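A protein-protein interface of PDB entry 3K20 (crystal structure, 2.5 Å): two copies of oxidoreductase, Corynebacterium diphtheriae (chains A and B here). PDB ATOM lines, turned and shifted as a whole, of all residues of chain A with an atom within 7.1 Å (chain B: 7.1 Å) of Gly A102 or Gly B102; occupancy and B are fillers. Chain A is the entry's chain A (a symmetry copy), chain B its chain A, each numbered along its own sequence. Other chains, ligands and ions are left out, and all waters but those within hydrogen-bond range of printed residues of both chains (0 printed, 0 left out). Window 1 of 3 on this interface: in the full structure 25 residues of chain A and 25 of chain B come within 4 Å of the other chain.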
ATOM      1  N   MET A  67      -6.283  -4.386 -17.666  1.00  0.00           N
ATOM      2  CA  MET A  67      -5.169  -4.458 -16.732  1.00  0.00           C
ATOM      3  C   MET A  67      -5.057  -5.855 -16.132  1.00  0.00           C
ATOM      4  O   MET A  67      -3.958  -6.333 -15.854  1.00  0.00           O
ATOM      5  CB  MET A  67      -5.330  -3.422 -15.612  1.00  0.00           C
ATOM      6  CG  MET A  67      -5.147  -1.972 -16.065  1.00  0.00           C
ATOM      7  SD  MET A  67      -3.469  -1.620 -17.012  1.00  0.00           S
ATOM      8  CE  MET A  67      -2.492  -0.695 -15.625  1.00  0.00           C
ATOM      9  N   THR A  93      -5.710  16.403 -21.522  1.00  0.00           N
ATOM     10  CA  THR A  93      -5.716  15.867 -20.170  1.00  0.00           C
ATOM     11  C   THR A  93      -5.636  16.923 -19.091  1.00  0.00           C
ATOM     12  O   THR A  93      -5.117  18.019 -19.310  1.00  0.00           O
ATOM     13  CB  THR A  93      -4.521  14.902 -19.938  1.00  0.00           C
ATOM     14  OG1 THR A  93      -4.449  14.543 -18.549  1.00  0.00           O
ATOM     15  CG2 THR A  93      -3.204  15.569 -20.344  1.00  0.00           C
ATOM     16  N   PHE A  96      -2.800  16.350 -13.010  1.00  0.00           N
ATOM     17  CA  PHE A  96      -2.857  15.774 -11.668  1.00  0.00           C
ATOM     18  C   PHE A  96      -1.429  15.548 -11.218  1.00  0.00           C
ATOM     19  O   PHE A  96      -0.618  15.017 -11.969  1.00  0.00           O
ATOM     20  CB  PHE A  96      -3.582  14.418 -11.671  1.00  0.00           C
ATOM     21  CG  PHE A  96      -5.071  14.505 -11.882  1.00  0.00           C
ATOM     22  CD1 PHE A  96      -5.723  15.741 -11.920  1.00  0.00           C
ATOM     23  CD2 PHE A  96      -5.829  13.340 -12.007  1.00  0.00           C
ATOM     24  CE1 PHE A  96      -7.112  15.815 -12.079  1.00  0.00           C
ATOM     25  CE2 PHE A  96      -7.224  13.402 -12.165  1.00  0.00           C
ATOM     26  CZ  PHE A  96      -7.864  14.646 -12.202  1.00  0.00           C
ATOM     27  N   SER A  99       1.383  16.606 -13.718  1.00  0.00           N
ATOM     28  CA  SER A  99       1.591  15.865 -14.960  1.00  0.00           C
ATOM     29  C   SER A  99       0.291  15.282 -15.511  1.00  0.00           C
ATOM     30  O   SER A  99      -0.796  15.584 -15.008  1.00  0.00           O
ATOM     31  CB  SER A  99       2.604  14.743 -14.745  1.00  0.00           C
ATOM     32  OG  SER A  99       2.902  14.105 -15.980  1.00  0.00           O
ATOM     33  N   TYR A 100       0.383  14.449 -16.545  1.00  0.00           N
ATOM     34  CA  TYR A 100      -0.845  13.902 -17.074  1.00  0.00           C
ATOM     35  C   TYR A 100      -1.496  12.887 -16.133  1.00  0.00           C
ATOM     36  O   TYR A 100      -0.878  12.379 -15.185  1.00  0.00           O
ATOM     37  CB  TYR A 100      -0.659  13.317 -18.484  1.00  0.00           C
ATOM     38  CG  TYR A 100       0.493  12.360 -18.698  1.00  0.00           C
ATOM     39  CD1 TYR A 100       0.659  11.218 -17.913  1.00  0.00           C
ATOM     40  CD2 TYR A 100       1.377  12.553 -19.759  1.00  0.00           C
ATOM     41  CE1 TYR A 100       1.688  10.292 -18.192  1.00  0.00           C
ATOM     42  CE2 TYR A 100       2.390  11.645 -20.040  1.00  0.00           C
ATOM     43  CZ  TYR A 100       2.536  10.522 -19.263  1.00  0.00           C
ATOM     44  OH  TYR A 100       3.532   9.639 -19.584  1.00  0.00           O
ATOM     45  N   THR A 101      -2.765  12.615 -16.401  1.00  0.00           N
ATOM     46  CA  THR A 101      -3.552  11.704 -15.598  1.00  0.00           C
ATOM     47  C   THR A 101      -3.196  10.231 -15.783  1.00  0.00           C
ATOM     48  O   THR A 101      -2.871   9.786 -16.890  1.00  0.00           O
ATOM     49  CB  THR A 101      -5.058  11.947 -15.889  1.00  0.00           C
ATOM     50  OG1 THR A 101      -5.472  13.145 -15.212  1.00  0.00           O
ATOM     51  CG2 THR A 101      -5.912  10.777 -15.440  1.00  0.00           C
ATOM     52  N   GLY A 102      -3.244   9.488 -14.677  1.00  0.00           N
ATOM     53  CA  GLY A 102      -2.956   8.067 -14.718  1.00  0.00           C
ATOM     54  C   GLY A 102      -3.878   7.374 -15.706  1.00  0.00           C
ATOM     55  O   GLY A 102      -3.442   6.505 -16.459  1.00  0.00           O
ATOM     56  N   LEU A 103      -5.151   7.768 -15.712  1.00  0.00           N
ATOM     57  CA  LEU A 103      -6.124   7.179 -16.629  1.00  0.00           C
ATOM     58  C   LEU A 103      -5.720   7.465 -18.071  1.00  0.00           C
ATOM     59  O   LEU A 103      -5.858   6.607 -18.954  1.00  0.00           O
ATOM     60  CB  LEU A 103      -7.518   7.749 -16.368  1.00  0.00           C
ATOM     61  CG  LEU A 103      -8.624   7.278 -17.319  1.00  0.00           C
ATOM     62  CD1 LEU A 103      -8.842   5.769 -17.215  1.00  0.00           C
ATOM     63  CD2 LEU A 103      -9.898   8.018 -16.975  1.00  0.00           C
ATOM     64  N   PHE A 104      -5.224   8.677 -18.296  1.00  0.00           N
ATOM     65  CA  PHE A 104      -4.783   9.098 -19.618  1.00  0.00           C
ATOM     66  C   PHE A 104      -3.668   8.152 -20.085  1.00  0.00           C
ATOM     67  O   PHE A 104      -3.777   7.517 -21.139  1.00  0.00           O
ATOM     68  CB  PHE A 104      -4.280  10.549 -19.540  1.00  0.00           C
ATOM     69  CG  PHE A 104      -3.820  11.121 -20.857  1.00  0.00           C
ATOM     70  CD1 PHE A 104      -4.738  11.469 -21.843  1.00  0.00           C
ATOM     71  CD2 PHE A 104      -2.460  11.318 -21.111  1.00  0.00           C
ATOM     72  CE1 PHE A 104      -4.308  12.010 -23.065  1.00  0.00           C
ATOM     73  CE2 PHE A 104      -2.022  11.861 -22.334  1.00  0.00           C
ATOM     74  CZ  PHE A 104      -2.954  12.203 -23.309  1.00  0.00           C
ATOM     75  N   LYS A 105      -2.609   8.061 -19.280  1.00  0.00           N
ATOM     76  CA  LYS A 105      -1.457   7.211 -19.585  1.00  0.00           C
ATOM     77  C   LYS A 105      -1.885   5.765 -19.823  1.00  0.00           C
ATOM     78  O   LYS A 105      -1.464   5.130 -20.797  1.00  0.00           O
ATOM     79  CB  LYS A 105      -0.431   7.275 -18.440  1.00  0.00           C
ATOM     80  CG  LYS A 105       0.850   6.465 -18.665  1.00  0.00           C
ATOM     81  CD  LYS A 105       1.495   6.790 -20.012  1.00  0.00           C
ATOM     82  CE  LYS A 105       2.967   6.403 -20.048  1.00  0.00           C
ATOM     83  NZ  LYS A 105       3.184   4.994 -19.612  1.00  0.00           N
ATOM     84  N   MET A 106      -2.737   5.262 -18.935  1.00  0.00           N
ATOM     85  CA  MET A 106      -3.231   3.893 -19.025  1.00  0.00           C
ATOM     86  C   MET A 106      -3.828   3.582 -20.393  1.00  0.00           C
ATOM     87  O   MET A 106      -3.622   2.496 -20.942  1.00  0.00           O
ATOM     88  CB  MET A 106      -4.285   3.644 -17.951  1.00  0.00           C
ATOM     89  CG  MET A 106      -4.701   2.195 -17.848  1.00  0.00           C
ATOM     90  SD  MET A 106      -6.051   1.933 -16.484  1.00  0.00           S
ATOM     91  CE  MET A 106      -5.071   2.480 -14.892  1.00  0.00           C
ATOM     92  N   PHE A 107      -4.578   4.533 -20.941  1.00  0.00           N
ATOM     93  CA  PHE A 107      -5.175   4.333 -22.248  1.00  0.00           C
ATOM     94  C   PHE A 107      -4.074   4.074 -23.278  1.00  0.00           C
ATOM     95  O   PHE A 107      -4.175   3.170 -24.109  1.00  0.00           O
ATOM     96  CB  PHE A 107      -5.981   5.562 -22.667  1.00  0.00           C
ATOM     97  CG  PHE A 107      -6.569   5.435 -24.034  1.00  0.00           C
ATOM     98  CD1 PHE A 107      -7.724   4.683 -24.240  1.00  0.00           C
ATOM     99  CD2 PHE A 107      -5.919   5.989 -25.130  1.00  0.00           C
ATOM    100  CE1 PHE A 107      -8.219   4.479 -25.524  1.00  0.00           C
ATOM    101  CE2 PHE A 107      -6.404   5.792 -26.425  1.00  0.00           C
ATOM    102  CZ  PHE A 107      -7.553   5.036 -26.621  1.00  0.00           C
ATOM    103  N   PHE A 108      -3.022   4.880 -23.219  1.00  0.00           N
ATOM    104  CA  PHE A 108      -1.909   4.720 -24.140  1.00  0.00           C
ATOM    105  C   PHE A 108      -1.108   3.446 -23.854  1.00  0.00           C
ATOM    106  O   PHE A 108      -0.567   2.832 -24.775  1.00  0.00           O
ATOM    107  CB  PHE A 108      -1.010   5.959 -24.095  1.00  0.00           C
ATOM    108  CG  PHE A 108      -1.632   7.161 -24.732  1.00  0.00           C
ATOM    109  CD1 PHE A 108      -1.566   7.345 -26.112  1.00  0.00           C
ATOM    110  CD2 PHE A 108      -2.375   8.062 -23.971  1.00  0.00           C
ATOM    111  CE1 PHE A 108      -2.242   8.407 -26.731  1.00  0.00           C
ATOM    112  CE2 PHE A 108      -3.056   9.126 -24.579  1.00  0.00           C
ATOM    113  CZ  PHE A 108      -2.988   9.294 -25.962  1.00  0.00           C
ATOM    114  N   ASP A 109      -1.033   3.042 -22.590  1.00  0.00           N
ATOM    115  CA  ASP A 109      -0.303   1.827 -22.255  1.00  0.00           C
ATOM    116  C   ASP A 109      -0.940   0.648 -22.974  1.00  0.00           C
ATOM    117  O   ASP A 109      -0.259  -0.237 -23.488  1.00  0.00           O
ATOM    118  CB  ASP A 109      -0.337   1.573 -20.750  1.00  0.00           C
ATOM    119  CG  ASP A 109       0.410   2.624 -19.972  1.00  0.00           C
ATOM    120  OD1 ASP A 109       1.341   3.235 -20.541  1.00  0.00           O
ATOM    121  OD2 ASP A 109       0.081   2.827 -18.786  1.00  0.00           O
ATOM    122  N   MET B  67     -12.095   6.658  -9.311  1.00  0.00           N
ATOM    123  CA  MET B  67     -12.147   7.487 -10.507  1.00  0.00           C
ATOM    124  C   MET B  67     -13.574   7.948 -10.785  1.00  0.00           C
ATOM    125  O   MET B  67     -13.793   9.053 -11.278  1.00  0.00           O
ATOM    126  CB  MET B  67     -11.602   6.726 -11.722  1.00  0.00           C
ATOM    127  CG  MET B  67     -10.091   6.481 -11.686  1.00  0.00           C
ATOM    128  SD  MET B  67      -9.013   8.094 -11.417  1.00  0.00           S
ATOM    129  CE  MET B  67      -8.338   8.345 -13.210  1.00  0.00           C
ATOM    130  N   THR B  93       8.162   0.710 -10.579  1.00  0.00           N
ATOM    131  CA  THR B  93       7.250   0.590 -11.705  1.00  0.00           C
ATOM    132  C   THR B  93       7.892   0.048 -12.964  1.00  0.00           C
ATOM    133  O   THR B  93       9.100   0.183 -13.169  1.00  0.00           O
ATOM    134  CB  THR B  93       6.628   1.965 -12.079  1.00  0.00           C
ATOM    135  OG1 THR B  93       5.887   1.846 -13.303  1.00  0.00           O
ATOM    136  CG2 THR B  93       7.725   3.016 -12.267  1.00  0.00           C
ATOM    137  N   PHE B  96       6.245   1.469 -19.337  1.00  0.00           N
ATOM    138  CA  PHE B  96       5.284   1.320 -20.428  1.00  0.00           C
ATOM    139  C   PHE B  96       5.331   2.597 -21.241  1.00  0.00           C
ATOM    140  O   PHE B  96       5.308   3.689 -20.684  1.00  0.00           O
ATOM    141  CB  PHE B  96       3.854   1.141 -19.896  1.00  0.00           C
ATOM    142  CG  PHE B  96       3.589  -0.196 -19.253  1.00  0.00           C
ATOM    143  CD1 PHE B  96       4.543  -1.216 -19.288  1.00  0.00           C
ATOM    144  CD2 PHE B  96       2.361  -0.446 -18.639  1.00  0.00           C
ATOM    145  CE1 PHE B  96       4.279  -2.469 -18.723  1.00  0.00           C
ATOM    146  CE2 PHE B  96       2.082  -1.700 -18.068  1.00  0.00           C
ATOM    147  CZ  PHE B  96       3.048  -2.713 -18.113  1.00  0.00           C
ATOM    148  N   SER B  99       7.851   5.338 -20.052  1.00  0.00           N
ATOM    149  CA  SER B  99       7.625   6.066 -18.807  1.00  0.00           C
ATOM    150  C   SER B  99       6.911   5.214 -17.759  1.00  0.00           C
ATOM    151  O   SER B  99       6.728   4.007 -17.951  1.00  0.00           O
ATOM    152  CB  SER B  99       6.818   7.334 -19.072  1.00  0.00           C
ATOM    153  OG  SER B  99       6.707   8.105 -17.883  1.00  0.00           O
ATOM    154  N   TYR B 100       6.503   5.822 -16.647  1.00  0.00           N
ATOM    155  CA  TYR B 100       5.834   5.017 -15.653  1.00  0.00           C
ATOM    156  C   TYR B 100       4.437   4.573 -16.090  1.00  0.00           C
ATOM    157  O   TYR B 100       3.849   5.102 -17.045  1.00  0.00           O
ATOM    158  CB  TYR B 100       5.796   5.707 -14.279  1.00  0.00           C
ATOM    159  CG  TYR B 100       5.311   7.140 -14.230  1.00  0.00           C
ATOM    160  CD1 TYR B 100       4.073   7.517 -14.751  1.00  0.00           C
ATOM    161  CD2 TYR B 100       6.063   8.112 -13.571  1.00  0.00           C
ATOM    162  CE1 TYR B 100       3.603   8.842 -14.609  1.00  0.00           C
ATOM    163  CE2 TYR B 100       5.605   9.415 -13.426  1.00  0.00           C
ATOM    164  CZ  TYR B 100       4.381   9.771 -13.938  1.00  0.00           C
ATOM    165  OH  TYR B 100       3.954  11.059 -13.757  1.00  0.00           O
ATOM    166  N   THR B 101       3.925   3.576 -15.384  1.00  0.00           N
ATOM    167  CA  THR B 101       2.628   3.002 -15.674  1.00  0.00           C
ATOM    168  C   THR B 101       1.446   3.887 -15.285  1.00  0.00           C
ATOM    169  O   THR B 101       1.478   4.587 -14.267  1.00  0.00           O
ATOM    170  CB  THR B 101       2.525   1.614 -14.988  1.00  0.00           C
ATOM    171  OG1 THR B 101       3.287   0.664 -15.749  1.00  0.00           O
ATOM    172  CG2 THR B 101       1.086   1.150 -14.872  1.00  0.00           C
ATOM    173  N   GLY B 102       0.410   3.858 -16.125  1.00  0.00           N
ATOM    174  CA  GLY B 102      -0.789   4.630 -15.860  1.00  0.00           C
ATOM    175  C   GLY B 102      -1.362   4.258 -14.505  1.00  0.00           C
ATOM    176  O   GLY B 102      -1.796   5.129 -13.751  1.00  0.00           O
ATOM    177  N   LEU B 103      -1.353   2.964 -14.188  1.00  0.00           N
ATOM    178  CA  LEU B 103      -1.868   2.492 -12.904  1.00  0.00           C
ATOM    179  C   LEU B 103      -1.045   3.081 -11.763  1.00  0.00           C
ATOM    180  O   LEU B 103      -1.586   3.455 -10.713  1.00  0.00           O
ATOM    181  CB  LEU B 103      -1.817   0.966 -12.835  1.00  0.00           C
ATOM    182  CG  LEU B 103      -2.251   0.340 -11.505  1.00  0.00           C
ATOM    183  CD1 LEU B 103      -3.715   0.650 -11.196  1.00  0.00           C
ATOM    184  CD2 LEU B 103      -2.038  -1.156 -11.589  1.00  0.00           C
ATOM    185  N   PHE B 104       0.263   3.154 -11.982  1.00  0.00           N
ATOM    186  CA  PHE B 104       1.182   3.702 -10.996  1.00  0.00           C
ATOM    187  C   PHE B 104       0.777   5.153 -10.703  1.00  0.00           C
ATOM    188  O   PHE B 104       0.500   5.514  -9.555  1.00  0.00           O
ATOM    189  CB  PHE B 104       2.615   3.629 -11.550  1.00  0.00           C
ATOM    190  CG  PHE B 104       3.675   4.141 -10.606  1.00  0.00           C
ATOM    191  CD1 PHE B 104       4.047   3.404  -9.486  1.00  0.00           C
ATOM    192  CD2 PHE B 104       4.308   5.363 -10.843  1.00  0.00           C
ATOM    193  CE1 PHE B 104       5.040   3.876  -8.614  1.00  0.00           C
ATOM    194  CE2 PHE B 104       5.306   5.843  -9.973  1.00  0.00           C
ATOM    195  CZ  PHE B 104       5.666   5.094  -8.858  1.00  0.00           C
ATOM    196  N   LYS B 105       0.732   5.968 -11.757  1.00  0.00           N
ATOM    197  CA  LYS B 105       0.373   7.382 -11.648  1.00  0.00           C
ATOM    198  C   LYS B 105      -0.983   7.557 -10.970  1.00  0.00           C
ATOM    199  O   LYS B 105      -1.139   8.380 -10.062  1.00  0.00           O
ATOM    200  CB  LYS B 105       0.355   8.036 -13.041  1.00  0.00           C
ATOM    201  CG  LYS B 105       0.043   9.536 -13.054  1.00  0.00           C
ATOM    202  CD  LYS B 105       0.938  10.308 -12.086  1.00  0.00           C
ATOM    203  CE  LYS B 105       1.004  11.791 -12.429  1.00  0.00           C
ATOM    204  NZ  LYS B 105      -0.353  12.387 -12.583  1.00  0.00           N
ATOM    205  N   MET B 106      -1.954   6.761 -11.410  1.00  0.00           N
ATOM    206  CA  MET B 106      -3.306   6.816 -10.867  1.00  0.00           C
ATOM    207  C   MET B 106      -3.324   6.688  -9.347  1.00  0.00           C
ATOM    208  O   MET B 106      -4.081   7.382  -8.662  1.00  0.00           O
ATOM    209  CB  MET B 106      -4.159   5.706 -11.470  1.00  0.00           C
ATOM    210  CG  MET B 106      -5.623   5.815 -11.112  1.00  0.00           C
ATOM    211  SD  MET B 106      -6.661   4.376 -11.888  1.00  0.00           S
ATOM    212  CE  MET B 106      -6.393   4.718 -13.786  1.00  0.00           C
ATOM    213  N   PHE B 107      -2.494   5.795  -8.818  1.00  0.00           N
ATOM    214  CA  PHE B 107      -2.430   5.614  -7.381  1.00  0.00           C
ATOM    215  C   PHE B 107      -2.039   6.936  -6.717  1.00  0.00           C
ATOM    216  O   PHE B 107      -2.628   7.349  -5.717  1.00  0.00           O
ATOM    217  CB  PHE B 107      -1.404   4.542  -7.016  1.00  0.00           C
ATOM    218  CG  PHE B 107      -1.252   4.358  -5.542  1.00  0.00           C
ATOM    219  CD1 PHE B 107      -2.189   3.620  -4.820  1.00  0.00           C
ATOM    220  CD2 PHE B 107      -0.226   4.998  -4.857  1.00  0.00           C
ATOM    221  CE1 PHE B 107      -2.108   3.529  -3.434  1.00  0.00           C
ATOM    222  CE2 PHE B 107      -0.133   4.916  -3.466  1.00  0.00           C
ATOM    223  CZ  PHE B 107      -1.074   4.183  -2.755  1.00  0.00           C
ATOM    224  N   PHE B 108      -1.035   7.595  -7.281  1.00  0.00           N
ATOM    225  CA  PHE B 108      -0.586   8.869  -6.745  1.00  0.00           C
ATOM    226  C   PHE B 108      -1.612   9.982  -6.976  1.00  0.00           C
ATOM    227  O   PHE B 108      -1.731  10.896  -6.159  1.00  0.00           O
ATOM    228  CB  PHE B 108       0.774   9.238  -7.347  1.00  0.00           C
ATOM    229  CG  PHE B 108       1.895   8.391  -6.832  1.00  0.00           C
ATOM    230  CD1 PHE B 108       2.513   8.695  -5.620  1.00  0.00           C
ATOM    231  CD2 PHE B 108       2.270   7.228  -7.502  1.00  0.00           C
ATOM    232  CE1 PHE B 108       3.486   7.845  -5.074  1.00  0.00           C
ATOM    233  CE2 PHE B 108       3.240   6.370  -6.966  1.00  0.00           C
ATOM    234  CZ  PHE B 108       3.846   6.682  -5.748  1.00  0.00           C
ATOM    235  N   ASP B 109      -2.355   9.910  -8.076  1.00  0.00           N
ATOM    236  CA  ASP B 109      -3.363  10.927  -8.342  1.00  0.00           C
ATOM    237  C   ASP B 109      -4.384  10.924  -7.216  1.00  0.00           C
ATOM    238  O   ASP B 109      -4.839  11.970  -6.757  1.00  0.00           O
ATOM    239  CB  ASP B 109      -4.075  10.649  -9.663  1.00  0.00           C
ATOM    240  CG  ASP B 109      -3.158  10.783 -10.851  1.00  0.00           C
ATOM    241  OD1 ASP B 109      -2.168  11.541 -10.754  1.00  0.00           O
ATOM    242  OD2 ASP B 109      -3.437  10.147 -11.888  1.00  0.00           O
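O of Phe B96 is in hydrogen-bond range of NZ of Lys A105. The side-chain amino group (NZ) of Lys A105 lies within hydrogen-bond range of the backbone carbonyl oxygen (O) of Tyr B100 (2.7 Å). The side-chain carboxylate (OD2) of Asp A109 is in hydrogen-bond range of the backbone NH (N) of Gly B102 (2.9 Å). O of Phe A96 sits at hydrogen-bond distance from NZ of Lys B105 (2.7 Å). The side-chain amino group (NZ) of Lys B105 lies within hydrogen-bond range of the backbone carbonyl oxygen (O) of Tyr A100, at 2.7 Å. OD2 of Asp B109 sits at hydrogen-bond distance from N of Gly A102 (2.9 Å). The backbone carbonyl oxygen (O) of Gly B102 sits close to the backbone carbonyl oxygen (O) of Gly A102 (3.5 Å).
Phe A96 touches Asp B109, and with the chains exchanged Asp A109 touches Phe B96. Tyr A100 touches Lys B105, and with the chains exchanged Lys A105 touches Tyr B100. Thr A101 touches Asp B109, and with the chains exchanged Asp A109 touches Thr B101. Gly A102 touches its own counterpart, Gly B102. Positions printed for both chains: 67, 93, 96, 99, 100, 101, 102, 103, 104, 105, 106, 107, 108 and 109.
Hydrophobic or aromatic side chains of chain B that line the printed part of chain A: Met B67, Phe B96, Tyr B100, Leu B103 and Met B106. Printed residues of chain A that touch a printed residue of chain B: Met A67, Phe A96, Ser A99, Tyr A100, Thr A101, Gly A102, Leu A103, Lys A105, Met A106 and Asp A109. Hydrophobic or aromatic side chains of chain A within 4 Å of the printed part of chain B: Met A67, Phe A96, Tyr A100, Leu A103 and Met A106. Along chain A the printed residues that touch a printed residue of chain B span positions 67 to 109.
Among the printed residues, pairs that only touch across the chains: Met A67 with Leu B103 (3.3 Å), Phe A96 with Asp B109 (3.3 Å), Ser A99 with Tyr B100 (3.9 Å), Tyr A100 with Ser B99 (3.9 Å), Thr A101 with Asp B109 (3.9 Å), Gly A102 with Lys B105 (3.7 Å), Gly A102 with Met B106 (3.7 Å), Leu A103 with Met B67 (3.3 Å), Leu A103 with Met B106 (3.8 Å), Lys A105 with Gly B102 (3.7 Å), Met A106 with Gly B102 (3.7 Å), Met A106 with Leu B103 (3.8 Å), Met A106 with Met B106 (2.8 Å), Asp A109 with Phe B96 (3.3 Å) and Asp A109 with Thr B101 (3.9 Å).
N of Thr B101 sits at hydrogen-bond distance from OG1 of Thr B93, 3.3 Å away. The side-chain carboxylate (OD1) of Asp B109 is in salt-bridge range of the side-chain amino group (NZ) of Lys B105. N of Thr A101 sits at hydrogen-bond distance from OG1 of Thr A93 (3.3 Å). The side-chain amino group of Lys A105 is in salt-bridge range of the side-chain carboxylate of Asp A109 (2.7 Å).
Gly A102 touches four residues of chain B. Gly B102 touches just these residues of chain A: Gly A102 (3.3 Å), Lys A105 (3.7 Å), Met A106 (3.7 Å) and Asp A109 (2.9 Å). Of the printed residues of chain B, Ser A99 touches Tyr B100 (3.9 Å). Of the printed residues of chain A, Phe B96 touches Lys A105 and Asp A109. Of the printed residues of chain B, Met A67 touches Leu B103 (3.3 Å). Printed residues of chain A within 4 Å of Met B106: Gly A102 (3.7 Å), Leu A103 (3.8 Å) and Met A106 (2.8 Å). The nearest residue of chain B that does not touch Gly A102 is Leu B103 (4.7 Å).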
